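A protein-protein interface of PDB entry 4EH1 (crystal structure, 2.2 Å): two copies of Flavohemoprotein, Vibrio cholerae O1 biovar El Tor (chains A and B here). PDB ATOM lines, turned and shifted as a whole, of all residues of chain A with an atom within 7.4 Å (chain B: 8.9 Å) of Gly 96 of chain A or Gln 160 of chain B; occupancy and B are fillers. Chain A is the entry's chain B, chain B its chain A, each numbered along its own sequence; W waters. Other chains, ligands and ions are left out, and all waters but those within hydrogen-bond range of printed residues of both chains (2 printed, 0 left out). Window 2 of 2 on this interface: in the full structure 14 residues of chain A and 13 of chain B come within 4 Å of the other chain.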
ATOM      1  N   PHE A   6      27.253  11.412   7.845  1.00  0.00           N
ATOM      2  CA  PHE A   6      25.944  10.819   8.041  1.00  0.00           C
ATOM      3  C   PHE A   6      25.394  10.469   6.660  1.00  0.00           C
ATOM      4  O   PHE A   6      25.689  11.163   5.678  1.00  0.00           O
ATOM      5  CB  PHE A   6      25.021  11.786   8.767  1.00  0.00           C
ATOM      6  CG  PHE A   6      25.135  11.731  10.273  1.00  0.00           C
ATOM      7  CD1 PHE A   6      26.306  12.134  10.908  1.00  0.00           C
ATOM      8  CD2 PHE A   6      24.048  11.303  11.055  1.00  0.00           C
ATOM      9  CE1 PHE A   6      26.438  12.054  12.277  1.00  0.00           C
ATOM     10  CE2 PHE A   6      24.153  11.259  12.451  1.00  0.00           C
ATOM     11  CZ  PHE A   6      25.350  11.637  13.066  1.00  0.00           C
ATOM     12  N   VAL A   7      24.614   9.398   6.579  1.00  0.00           N
ATOM     13  CA  VAL A   7      23.995   9.044   5.314  1.00  0.00           C
ATOM     14  C   VAL A   7      22.488   9.268   5.369  1.00  0.00           C
ATOM     15  O   VAL A   7      21.879   9.164   6.437  1.00  0.00           O
ATOM     16  CB  VAL A   7      24.351   7.607   4.868  1.00  0.00           C
ATOM     17  CG1 VAL A   7      23.944   6.592   5.919  1.00  0.00           C
ATOM     18  CG2 VAL A   7      23.713   7.285   3.505  1.00  0.00           C
ATOM     19  N   VAL A   8      21.894   9.602   4.223  1.00  0.00           N
ATOM     20  CA  VAL A   8      20.466   9.887   4.169  1.00  0.00           C
ATOM     21  C   VAL A   8      19.737   8.554   4.094  1.00  0.00           C
ATOM     22  O   VAL A   8      19.932   7.807   3.153  1.00  0.00           O
ATOM     23  CB  VAL A   8      20.118  10.731   2.942  1.00  0.00           C
ATOM     24  CG1 VAL A   8      18.582  10.781   2.771  1.00  0.00           C
ATOM     25  CG2 VAL A   8      20.722  12.125   3.096  1.00  0.00           C
ATOM     26  N   ARG A   9      18.915   8.234   5.087  1.00  0.00           N
ATOM     27  CA  ARG A   9      18.238   6.937   5.055  1.00  0.00           C
ATOM     28  C   ARG A   9      16.852   7.113   4.421  1.00  0.00           C
ATOM     29  O   ARG A   9      16.303   6.179   3.848  1.00  0.00           O
ATOM     30  CB  ARG A   9      18.120   6.344   6.472  1.00  0.00           C
ATOM     31  CG  ARG A   9      17.502   4.948   6.505  1.00  0.00           C
ATOM     32  CD  ARG A   9      17.500   4.286   7.893  1.00  0.00           C
ATOM     33  NE  ARG A   9      16.682   5.009   8.870  1.00  0.00           N
ATOM     34  CZ  ARG A   9      15.372   4.828   9.054  1.00  0.00           C
ATOM     35  NH1 ARG A   9      14.709   3.935   8.324  1.00  0.00           N
ATOM     36  NH2 ARG A   9      14.719   5.541   9.971  1.00  0.00           N
ATOM     37  N   GLU A  10      16.261   8.304   4.560  1.00  0.00           N
ATOM     38  CA  GLU A  10      14.913   8.513   3.997  1.00  0.00           C
ATOM     39  C   GLU A  10      14.825   9.942   3.519  1.00  0.00           C
ATOM     40  O   GLU A  10      15.481  10.810   4.076  1.00  0.00           O
ATOM     41  CB  GLU A  10      13.814   8.241   5.049  1.00  0.00           C
ATOM     42  CG  GLU A  10      13.775   6.794   5.553  1.00  0.00           C
ATOM     43  CD  GLU A  10      12.842   6.581   6.753  1.00  0.00           C
ATOM     44  OE1 GLU A  10      11.987   7.455   7.017  1.00  0.00           O
ATOM     45  OE2 GLU A  10      12.966   5.534   7.437  1.00  0.00           O
ATOM     46  N   VAL A  93      20.982  15.461  -3.266  1.00  0.00           N
ATOM     47  CA  VAL A  93      21.309  14.585  -2.153  1.00  0.00           C
ATOM     48  C   VAL A  93      20.232  13.505  -2.030  1.00  0.00           C
ATOM     49  O   VAL A  93      19.132  13.732  -1.506  1.00  0.00           O
ATOM     50  CB  VAL A  93      21.518  15.403  -0.854  1.00  0.00           C
ATOM     51  CG1 VAL A  93      21.947  14.502   0.306  1.00  0.00           C
ATOM     52  CG2 VAL A  93      22.560  16.490  -1.090  1.00  0.00           C
ATOM     53  N   LYS A  94      20.567  12.329  -2.529  1.00  0.00           N
ATOM     54  CA  LYS A  94      19.618  11.232  -2.622  1.00  0.00           C
ATOM     55  C   LYS A  94      19.686  10.370  -1.342  1.00  0.00           C
ATOM     56  O   LYS A  94      20.666  10.451  -0.592  1.00  0.00           O
ATOM     57  CB  LYS A  94      19.984  10.348  -3.812  1.00  0.00           C
ATOM     58  CG  LYS A  94      19.938  11.024  -5.194  1.00  0.00           C
ATOM     59  CD  LYS A  94      20.145   9.993  -6.381  1.00  0.00           C
ATOM     60  CE  LYS A  94      21.521   9.302  -6.310  1.00  0.00           C
ATOM     61  NZ  LYS A  94      22.616  10.299  -5.999  1.00  0.00           N
ATOM     62  N   VAL A  95      18.651   9.563  -1.099  1.00  0.00           N
ATOM     63  CA  VAL A  95      18.780   8.438  -0.179  1.00  0.00           C
ATOM     64  C   VAL A  95      20.058   7.676  -0.555  1.00  0.00           C
ATOM     65  O   VAL A  95      20.315   7.428  -1.739  1.00  0.00           O
ATOM     66  CB  VAL A  95      17.565   7.489  -0.273  1.00  0.00           C
ATOM     67  CG1 VAL A  95      17.811   6.119   0.554  1.00  0.00           C
ATOM     68  CG2 VAL A  95      16.260   8.225   0.186  1.00  0.00           C
ATOM     69  N   GLY A  96      20.867   7.344   0.453  1.00  0.00           N
ATOM     70  CA  GLY A  96      22.127   6.671   0.219  1.00  0.00           C
ATOM     71  C   GLY A  96      23.298   7.638   0.081  1.00  0.00           C
ATOM     72  O   GLY A  96      24.436   7.213   0.093  1.00  0.00           O
ATOM     73  N   ASP A  97      23.050   8.938  -0.061  1.00  0.00           N
ATOM     74  CA  ASP A  97      24.181   9.856  -0.212  1.00  0.00           C
ATOM     75  C   ASP A  97      24.581  10.371   1.177  1.00  0.00           C
ATOM     76  O   ASP A  97      23.783  10.363   2.113  1.00  0.00           O
ATOM     77  CB  ASP A  97      23.855  11.025  -1.133  1.00  0.00           C
ATOM     78  CG  ASP A  97      23.705  10.613  -2.620  1.00  0.00           C
ATOM     79  OD1 ASP A  97      24.153   9.501  -3.001  1.00  0.00           O
ATOM     80  OD2 ASP A  97      23.135  11.426  -3.406  1.00  0.00           O
ATOM     81  N   SER A  98      25.811  10.839   1.318  1.00  0.00           N
ATOM     82  CA  SER A  98      26.236  11.328   2.621  1.00  0.00           C
ATOM     83  C   SER A  98      26.472  12.824   2.660  1.00  0.00           C
ATOM     84  O   SER A  98      26.588  13.465   1.619  1.00  0.00           O
ATOM     85  CB  SER A  98      27.460  10.568   3.098  1.00  0.00           C
ATOM     86  OG  SER A  98      28.383  10.484   2.063  1.00  0.00           O
ATOM     87  N   VAL B  13      11.222  10.877  -2.055  1.00  0.00           N
ATOM     88  CA  VAL B  13      11.975  11.344  -3.201  1.00  0.00           C
ATOM     89  C   VAL B  13      12.924  10.258  -3.634  1.00  0.00           C
ATOM     90  O   VAL B  13      13.733   9.800  -2.857  1.00  0.00           O
ATOM     91  CB  VAL B  13      12.760  12.618  -2.872  1.00  0.00           C
ATOM     92  CG1 VAL B  13      13.560  13.095  -4.094  1.00  0.00           C
ATOM     93  CG2 VAL B  13      11.794  13.686  -2.426  1.00  0.00           C
ATOM     94  N   GLU B  14      12.817   9.838  -4.884  1.00  0.00           N
ATOM     95  CA  GLU B  14      13.728   8.833  -5.399  1.00  0.00           C
ATOM     96  C   GLU B  14      14.925   9.443  -6.128  1.00  0.00           C
ATOM     97  O   GLU B  14      15.997   8.882  -6.093  1.00  0.00           O
ATOM     98  CB  GLU B  14      13.006   7.867  -6.344  1.00  0.00           C
ATOM     99  CG  GLU B  14      11.844   7.145  -5.723  1.00  0.00           C
ATOM    100  CD  GLU B  14      12.286   6.164  -4.612  1.00  0.00           C
ATOM    101  OE1 GLU B  14      13.510   6.047  -4.343  1.00  0.00           O
ATOM    102  OE2 GLU B  14      11.401   5.488  -4.025  1.00  0.00           O
ATOM    103  N   GLN B 130      11.876  -2.152 -10.987  1.00  0.00           N
ATOM    104  CA  GLN B 130      11.981  -2.233  -9.537  1.00  0.00           C
ATOM    105  C   GLN B 130      11.012  -3.259  -8.895  1.00  0.00           C
ATOM    106  O   GLN B 130      11.373  -3.940  -7.927  1.00  0.00           O
ATOM    107  CB  GLN B 130      11.795  -0.849  -8.912  1.00  0.00           C
ATOM    108  CG  GLN B 130      12.596  -0.679  -7.592  1.00  0.00           C
ATOM    109  CD  GLN B 130      14.118  -0.710  -7.800  1.00  0.00           C
ATOM    110  OE1 GLN B 130      14.623  -0.654  -8.932  1.00  0.00           O
ATOM    111  NE2 GLN B 130      14.848  -0.813  -6.707  1.00  0.00           N
ATOM    112  N   HIS B 134      12.340  -6.588  -6.839  1.00  0.00           N
ATOM    113  CA  HIS B 134      11.854  -6.967  -5.514  1.00  0.00           C
ATOM    114  C   HIS B 134      11.212  -8.353  -5.486  1.00  0.00           C
ATOM    115  O   HIS B 134      11.388  -9.108  -4.511  1.00  0.00           O
ATOM    116  CB  HIS B 134      10.912  -5.924  -4.926  1.00  0.00           C
ATOM    117  CG  HIS B 134      11.616  -4.738  -4.351  1.00  0.00           C
ATOM    118  ND1 HIS B 134      12.423  -4.824  -3.233  1.00  0.00           N
ATOM    119  CD2 HIS B 134      11.631  -3.435  -4.731  1.00  0.00           C
ATOM    120  CE1 HIS B 134      12.898  -3.624  -2.942  1.00  0.00           C
ATOM    121  NE2 HIS B 134      12.446  -2.768  -3.847  1.00  0.00           N
ATOM    122  N   ALA B 153      24.106  11.458 -11.810  1.00  0.00           N
ATOM    123  CA  ALA B 153      23.959  10.985 -10.446  1.00  0.00           C
ATOM    124  C   ALA B 153      22.644  11.474  -9.853  1.00  0.00           C
ATOM    125  O   ALA B 153      21.913  10.695  -9.235  1.00  0.00           O
ATOM    126  CB  ALA B 153      25.174  11.415  -9.549  1.00  0.00           C
ATOM    127  N   HIS B 156      19.652   9.379 -10.769  1.00  0.00           N
ATOM    128  CA  HIS B 156      19.873   7.942 -10.696  1.00  0.00           C
ATOM    129  C   HIS B 156      18.791   7.303  -9.787  1.00  0.00           C
ATOM    130  O   HIS B 156      19.012   7.090  -8.597  1.00  0.00           O
ATOM    131  CB  HIS B 156      21.280   7.691 -10.143  1.00  0.00           C
ATOM    132  CG  HIS B 156      21.684   6.248 -10.107  1.00  0.00           C
ATOM    133  ND1 HIS B 156      22.986   5.845  -9.858  1.00  0.00           N
ATOM    134  CD2 HIS B 156      20.966   5.114 -10.265  1.00  0.00           C
ATOM    135  CE1 HIS B 156      23.050   4.528  -9.891  1.00  0.00           C
ATOM    136  NE2 HIS B 156      21.837   4.058 -10.134  1.00  0.00           N
ATOM    137  N   THR B 157      17.632   6.999 -10.357  1.00  0.00           N
ATOM    138  CA  THR B 157      16.486   6.545  -9.580  1.00  0.00           C
ATOM    139  C   THR B 157      16.699   5.207  -8.872  1.00  0.00           C
ATOM    140  O   THR B 157      17.180   4.266  -9.479  1.00  0.00           O
ATOM    141  CB  THR B 157      15.294   6.419 -10.529  1.00  0.00           C
ATOM    142  OG1 THR B 157      15.083   7.688 -11.166  1.00  0.00           O
ATOM    143  CG2 THR B 157      14.017   5.957  -9.781  1.00  0.00           C
ATOM    144  N   PHE B 158      16.336   5.130  -7.591  1.00  0.00           N
ATOM    145  CA  PHE B 158      16.490   3.923  -6.787  1.00  0.00           C
ATOM    146  C   PHE B 158      17.931   3.519  -6.537  1.00  0.00           C
ATOM    147  O   PHE B 158      18.177   2.336  -6.273  1.00  0.00           O
ATOM    148  CB  PHE B 158      15.793   2.724  -7.449  1.00  0.00           C
ATOM    149  CG  PHE B 158      14.333   2.923  -7.671  1.00  0.00           C
ATOM    150  CD1 PHE B 158      13.513   3.303  -6.631  1.00  0.00           C
ATOM    151  CD2 PHE B 158      13.778   2.742  -8.936  1.00  0.00           C
ATOM    152  CE1 PHE B 158      12.136   3.472  -6.846  1.00  0.00           C
ATOM    153  CE2 PHE B 158      12.405   2.928  -9.158  1.00  0.00           C
ATOM    154  CZ  PHE B 158      11.599   3.293  -8.111  1.00  0.00           C
ATOM    155  N   ALA B 159      18.879   4.463  -6.626  1.00  0.00           N
ATOM    156  CA  ALA B 159      20.297   4.089  -6.583  1.00  0.00           C
ATOM    157  C   ALA B 159      20.575   3.202  -5.358  1.00  0.00           C
ATOM    158  O   ALA B 159      21.142   2.122  -5.477  1.00  0.00           O
ATOM    159  CB  ALA B 159      21.198   5.319  -6.538  1.00  0.00           C
ATOM    160  N   GLN B 160      20.142   3.662  -4.191  1.00  0.00           N
ATOM    161  CA  GLN B 160      20.466   2.988  -2.935  1.00  0.00           C
ATOM    162  C   GLN B 160      19.705   1.668  -2.770  1.00  0.00           C
ATOM    163  O   GLN B 160      20.267   0.654  -2.377  1.00  0.00           O
ATOM    164  CB  GLN B 160      20.178   3.906  -1.740  1.00  0.00           C
ATOM    165  CG  GLN B 160      20.379   3.229  -0.385  1.00  0.00           C
ATOM    166  CD  GLN B 160      21.834   2.797  -0.169  1.00  0.00           C
ATOM    167  OE1 GLN B 160      22.745   3.237  -0.877  1.00  0.00           O
ATOM    168  NE2 GLN B 160      22.053   1.943   0.819  1.00  0.00           N
ATOM    169  N   GLU B 161      18.426   1.695  -3.097  1.00  0.00           N
ATOM    170  CA  GLU B 161      17.586   0.545  -2.884  1.00  0.00           C
ATOM    171  C   GLU B 161      18.058  -0.592  -3.785  1.00  0.00           C
ATOM    172  O   GLU B 161      18.146  -1.731  -3.352  1.00  0.00           O
ATOM    173  CB  GLU B 161      16.126   0.931  -3.120  1.00  0.00           C
ATOM    174  CG  GLU B 161      15.087  -0.188  -2.953  1.00  0.00           C
ATOM    175  CD  GLU B 161      13.654   0.309  -3.277  1.00  0.00           C
ATOM    176  OE1 GLU B 161      13.114   0.017  -4.364  1.00  0.00           O
ATOM    177  OE2 GLU B 161      13.069   1.002  -2.435  1.00  0.00           O
ATOM    178  N   THR B 162      18.399  -0.261  -5.022  1.00  0.00           N
ATOM    179  CA  THR B 162      18.873  -1.253  -5.969  1.00  0.00           C
ATOM    180  C   THR B 162      20.238  -1.819  -5.553  1.00  0.00           C
ATOM    181  O   THR B 162      20.461  -3.022  -5.631  1.00  0.00           O
ATOM    182  CB  THR B 162      18.894  -0.653  -7.393  1.00  0.00           C
ATOM    183  OG1 THR B 162      17.548  -0.388  -7.782  1.00  0.00           O
ATOM    184  CG2 THR B 162      19.518  -1.596  -8.426  1.00  0.00           C
ATOM    185  N   ALA B 163      21.132  -0.953  -5.091  1.00  0.00           N
ATOM    186  CA  ALA B 163      22.460  -1.374  -4.664  1.00  0.00           C
ATOM    187  C   ALA B 163      22.311  -2.397  -3.544  1.00  0.00           C
ATOM    188  O   ALA B 163      22.993  -3.417  -3.529  1.00  0.00           O
ATOM    189  CB  ALA B 163      23.292  -0.176  -4.169  1.00  0.00           C
ATOM    190  N   GLN B 164      21.399  -2.125  -2.620  1.00  0.00           N
ATOM    191  CA  GLN B 164      21.194  -3.034  -1.500  1.00  0.00           C
ATOM    192  C   GLN B 164      20.703  -4.398  -1.967  1.00  0.00           C
ATOM    193  O   GLN B 164      21.243  -5.413  -1.536  1.00  0.00           O
ATOM    194  CB  GLN B 164      20.260  -2.436  -0.448  1.00  0.00           C
ATOM    195  CG  GLN B 164      20.834  -1.206   0.242  1.00  0.00           C
ATOM    196  CD  GLN B 164      20.096  -0.870   1.542  1.00  0.00           C
ATOM    197  OE1 GLN B 164      19.914   0.308   1.899  1.00  0.00           O
ATOM    198  NE2 GLN B 164      19.671  -1.915   2.258  1.00  0.00           N
ATOM    199  N   LEU B 165      19.703  -4.416  -2.849  1.00  0.00           N
ATOM    200  CA  LEU B 165      19.177  -5.676  -3.380  1.00  0.00           C
ATOM    201  C   LEU B 165      20.274  -6.449  -4.023  1.00  0.00           C
ATOM    202  O   LEU B 165      20.459  -7.625  -3.751  1.00  0.00           O
ATOM    203  CB  LEU B 165      18.094  -5.453  -4.430  1.00  0.00           C
ATOM    204  CG  LEU B 165      16.720  -5.105  -3.868  1.00  0.00           C
ATOM    205  CD1 LEU B 165      15.714  -4.798  -4.978  1.00  0.00           C
ATOM    206  CD2 LEU B 165      16.209  -6.239  -2.929  1.00  0.00           C
ATOM    207  N   ILE B 166      21.015  -5.767  -4.881  1.00  0.00           N
ATOM    208  CA  ILE B 166      22.105  -6.411  -5.584  1.00  0.00           C
ATOM    209  C   ILE B 166      23.115  -6.974  -4.625  1.00  0.00           C
ATOM    210  O   ILE B 166      23.528  -8.114  -4.776  1.00  0.00           O
ATOM    211  CB  ILE B 166      22.759  -5.458  -6.624  1.00  0.00           C
ATOM    212  CG1 ILE B 166      21.899  -5.494  -7.880  1.00  0.00           C
ATOM    213  CG2 ILE B 166      24.147  -5.949  -7.001  1.00  0.00           C
ATOM    214  CD1 ILE B 166      21.644  -4.219  -8.436  1.00  0.00           C
ATOM    215  N   ALA B 167      23.487  -6.181  -3.621  1.00  0.00           N
ATOM    216  CA  ALA B 167      24.437  -6.617  -2.618  1.00  0.00           C
ATOM    217  C   ALA B 167      23.877  -7.760  -1.785  1.00  0.00           C
ATOM    218  O   ALA B 167      24.634  -8.541  -1.257  1.00  0.00           O
ATOM    219  CB  ALA B 167      24.848  -5.456  -1.694  1.00  0.00           C
ATOM    220  N   GLN B 168      22.559  -7.851  -1.671  1.00  0.00           N
ATOM    221  CA  GLN B 168      21.941  -8.914  -0.890  1.00  0.00           C
ATOM    222  C   GLN B 168      21.758 -10.208  -1.661  1.00  0.00           C
ATOM    223  O   GLN B 168      21.902 -11.274  -1.070  1.00  0.00           O
ATOM    224  CB  GLN B 168      20.592  -8.481  -0.332  1.00  0.00           C
ATOM    225  CG  GLN B 168      20.721  -7.609   0.887  1.00  0.00           C
ATOM    226  CD  GLN B 168      19.404  -6.973   1.277  1.00  0.00           C
ATOM    227  OE1 GLN B 168      18.330  -7.500   0.967  1.00  0.00           O
ATOM    228  NE2 GLN B 168      19.476  -5.827   1.948  1.00  0.00           N
ATOM    229  N   GLN B 173      25.107  -5.615 -11.696  1.00  0.00           N
ATOM    230  CA  GLN B 173      24.550  -4.415 -12.290  1.00  0.00           C
ATOM    231  C   GLN B 173      25.629  -3.583 -12.986  1.00  0.00           C
ATOM    232  O   GLN B 173      26.813  -3.619 -12.603  1.00  0.00           O
ATOM    233  CB  GLN B 173      23.736  -3.597 -11.273  1.00  0.00           C
ATOM    234  CG  GLN B 173      24.498  -2.516 -10.497  1.00  0.00           C
ATOM    235  CD  GLN B 173      23.548  -1.477  -9.845  1.00  0.00           C
ATOM    236  OE1 GLN B 173      22.651  -0.939 -10.495  1.00  0.00           O
ATOM    237  NE2 GLN B 173      23.763  -1.195  -8.568  1.00  0.00           N
ATOM    238  N   TYR B 177      25.806   6.866 -17.102  1.00  0.00           N
ATOM    239  CA  TYR B 177      25.345   8.248 -16.939  1.00  0.00           C
ATOM    240  C   TYR B 177      25.620   8.910 -18.269  1.00  0.00           C
ATOM    241  O   TYR B 177      26.758   8.878 -18.776  1.00  0.00           O
ATOM    242  CB  TYR B 177      26.115   8.995 -15.841  1.00  0.00           C
ATOM    243  CG  TYR B 177      25.822   8.616 -14.393  1.00  0.00           C
ATOM    244  CD1 TYR B 177      24.716   7.828 -14.048  1.00  0.00           C
ATOM    245  CD2 TYR B 177      26.651   9.077 -13.359  1.00  0.00           C
ATOM    246  CE1 TYR B 177      24.454   7.496 -12.708  1.00  0.00           C
ATOM    247  CE2 TYR B 177      26.405   8.741 -12.025  1.00  0.00           C
ATOM    248  CZ  TYR B 177      25.293   7.942 -11.708  1.00  0.00           C
ATOM    249  OH  TYR B 177      25.029   7.612 -10.378  1.00  0.00           O
HETATM  250  O   HOH W   1      18.866   6.209  -3.657  1.00  0.00           O
HETATM  251  O   HOH W   2      16.460   9.730  -3.299  1.00  0.00           O
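NZ of Lys 94 of chain A sits close to O of Ala 153 of chain B.
OH of Tyr 177 of chain B lies within hydrogen-bond range of ND1 of His 156 of chain B (2.8 Å). NE2 of Gln 160 of chain B lies within hydrogen-bond range of OE1 of Gln 164 of chain B, at 2.9 Å. O of Val 8 of chain A is in hydrogen-bond range of N of Gly 96 of chain A (2.9 Å). NZ of Lys 94 of chain A is in salt-bridge range of OD2 of Asp 97 of chain A (2.9 Å).
Lys 94 of chain A touches His 156 of chain B. Gln 160 of chain B touches Val 95 of chain A (CB to O, 3.5 Å). Gln 160 of chain B touches Gly 96 of chain A.
Of chain B, only Gln 160 (3.7 Å) comes within 4 Å of Gly 96 of chain A. Of the printed residues of chain A, Gln 160 of chain B touches Val 95 (3.5 Å) and Gly 96 (3.7 Å). Printed residues of chain A within 4 Å of Ala 153 of chain B: Lys 94 (3.3 Å). Of the printed residues of chain A, His 156 of chain B touches Lys 94. Of the printed residues of chain B, Lys 94 of chain A touches Ala 153 and His 156. Val 13 of chain B touches none of the printed residues of chain A. Arg 9 of chain A touches none of the printed residues of chain B. The nearest residue of chain A that does not touch Gln 160 of chain B is Asp 97 of chain A (5.8 Å). The nearest printed residue of chain B that does not touch Lys 94 of chain A is Ala 159 of chain B (4.003 Å).
Of the 11 printed residues of chain A, 3 touch a printed residue of chain B. Printed residues of chain A that touch a printed residue of chain B: Lys 94, Val 95 and Gly 96. Hydrophobic or aromatic side chains of chain A that line the printed part of chain B: Val 95. Of the 20 printed residues of chain B, 3 touch a printed residue of chain A. Among the printed residues, 4 pairs touch across the chains.
No position is printed for both chains. Of the 4 pairs that touch across the chains among the printed residues, none has its exchanged pair printed and touching as well.
Water W1 lies within hydrogen-bond range of the backbone carbonyl oxygen of Val 95 of chain A, the backbone NH of Gln 160 of chain B and the backbone NH of Ala 159 of chain B. Water W2 lies within hydrogen-bond range of O of Val 13 of chain B (2.8 Å), O of Glu 14 of chain B (3.0 Å) and N of Val 95 of chain A (3.1 Å).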
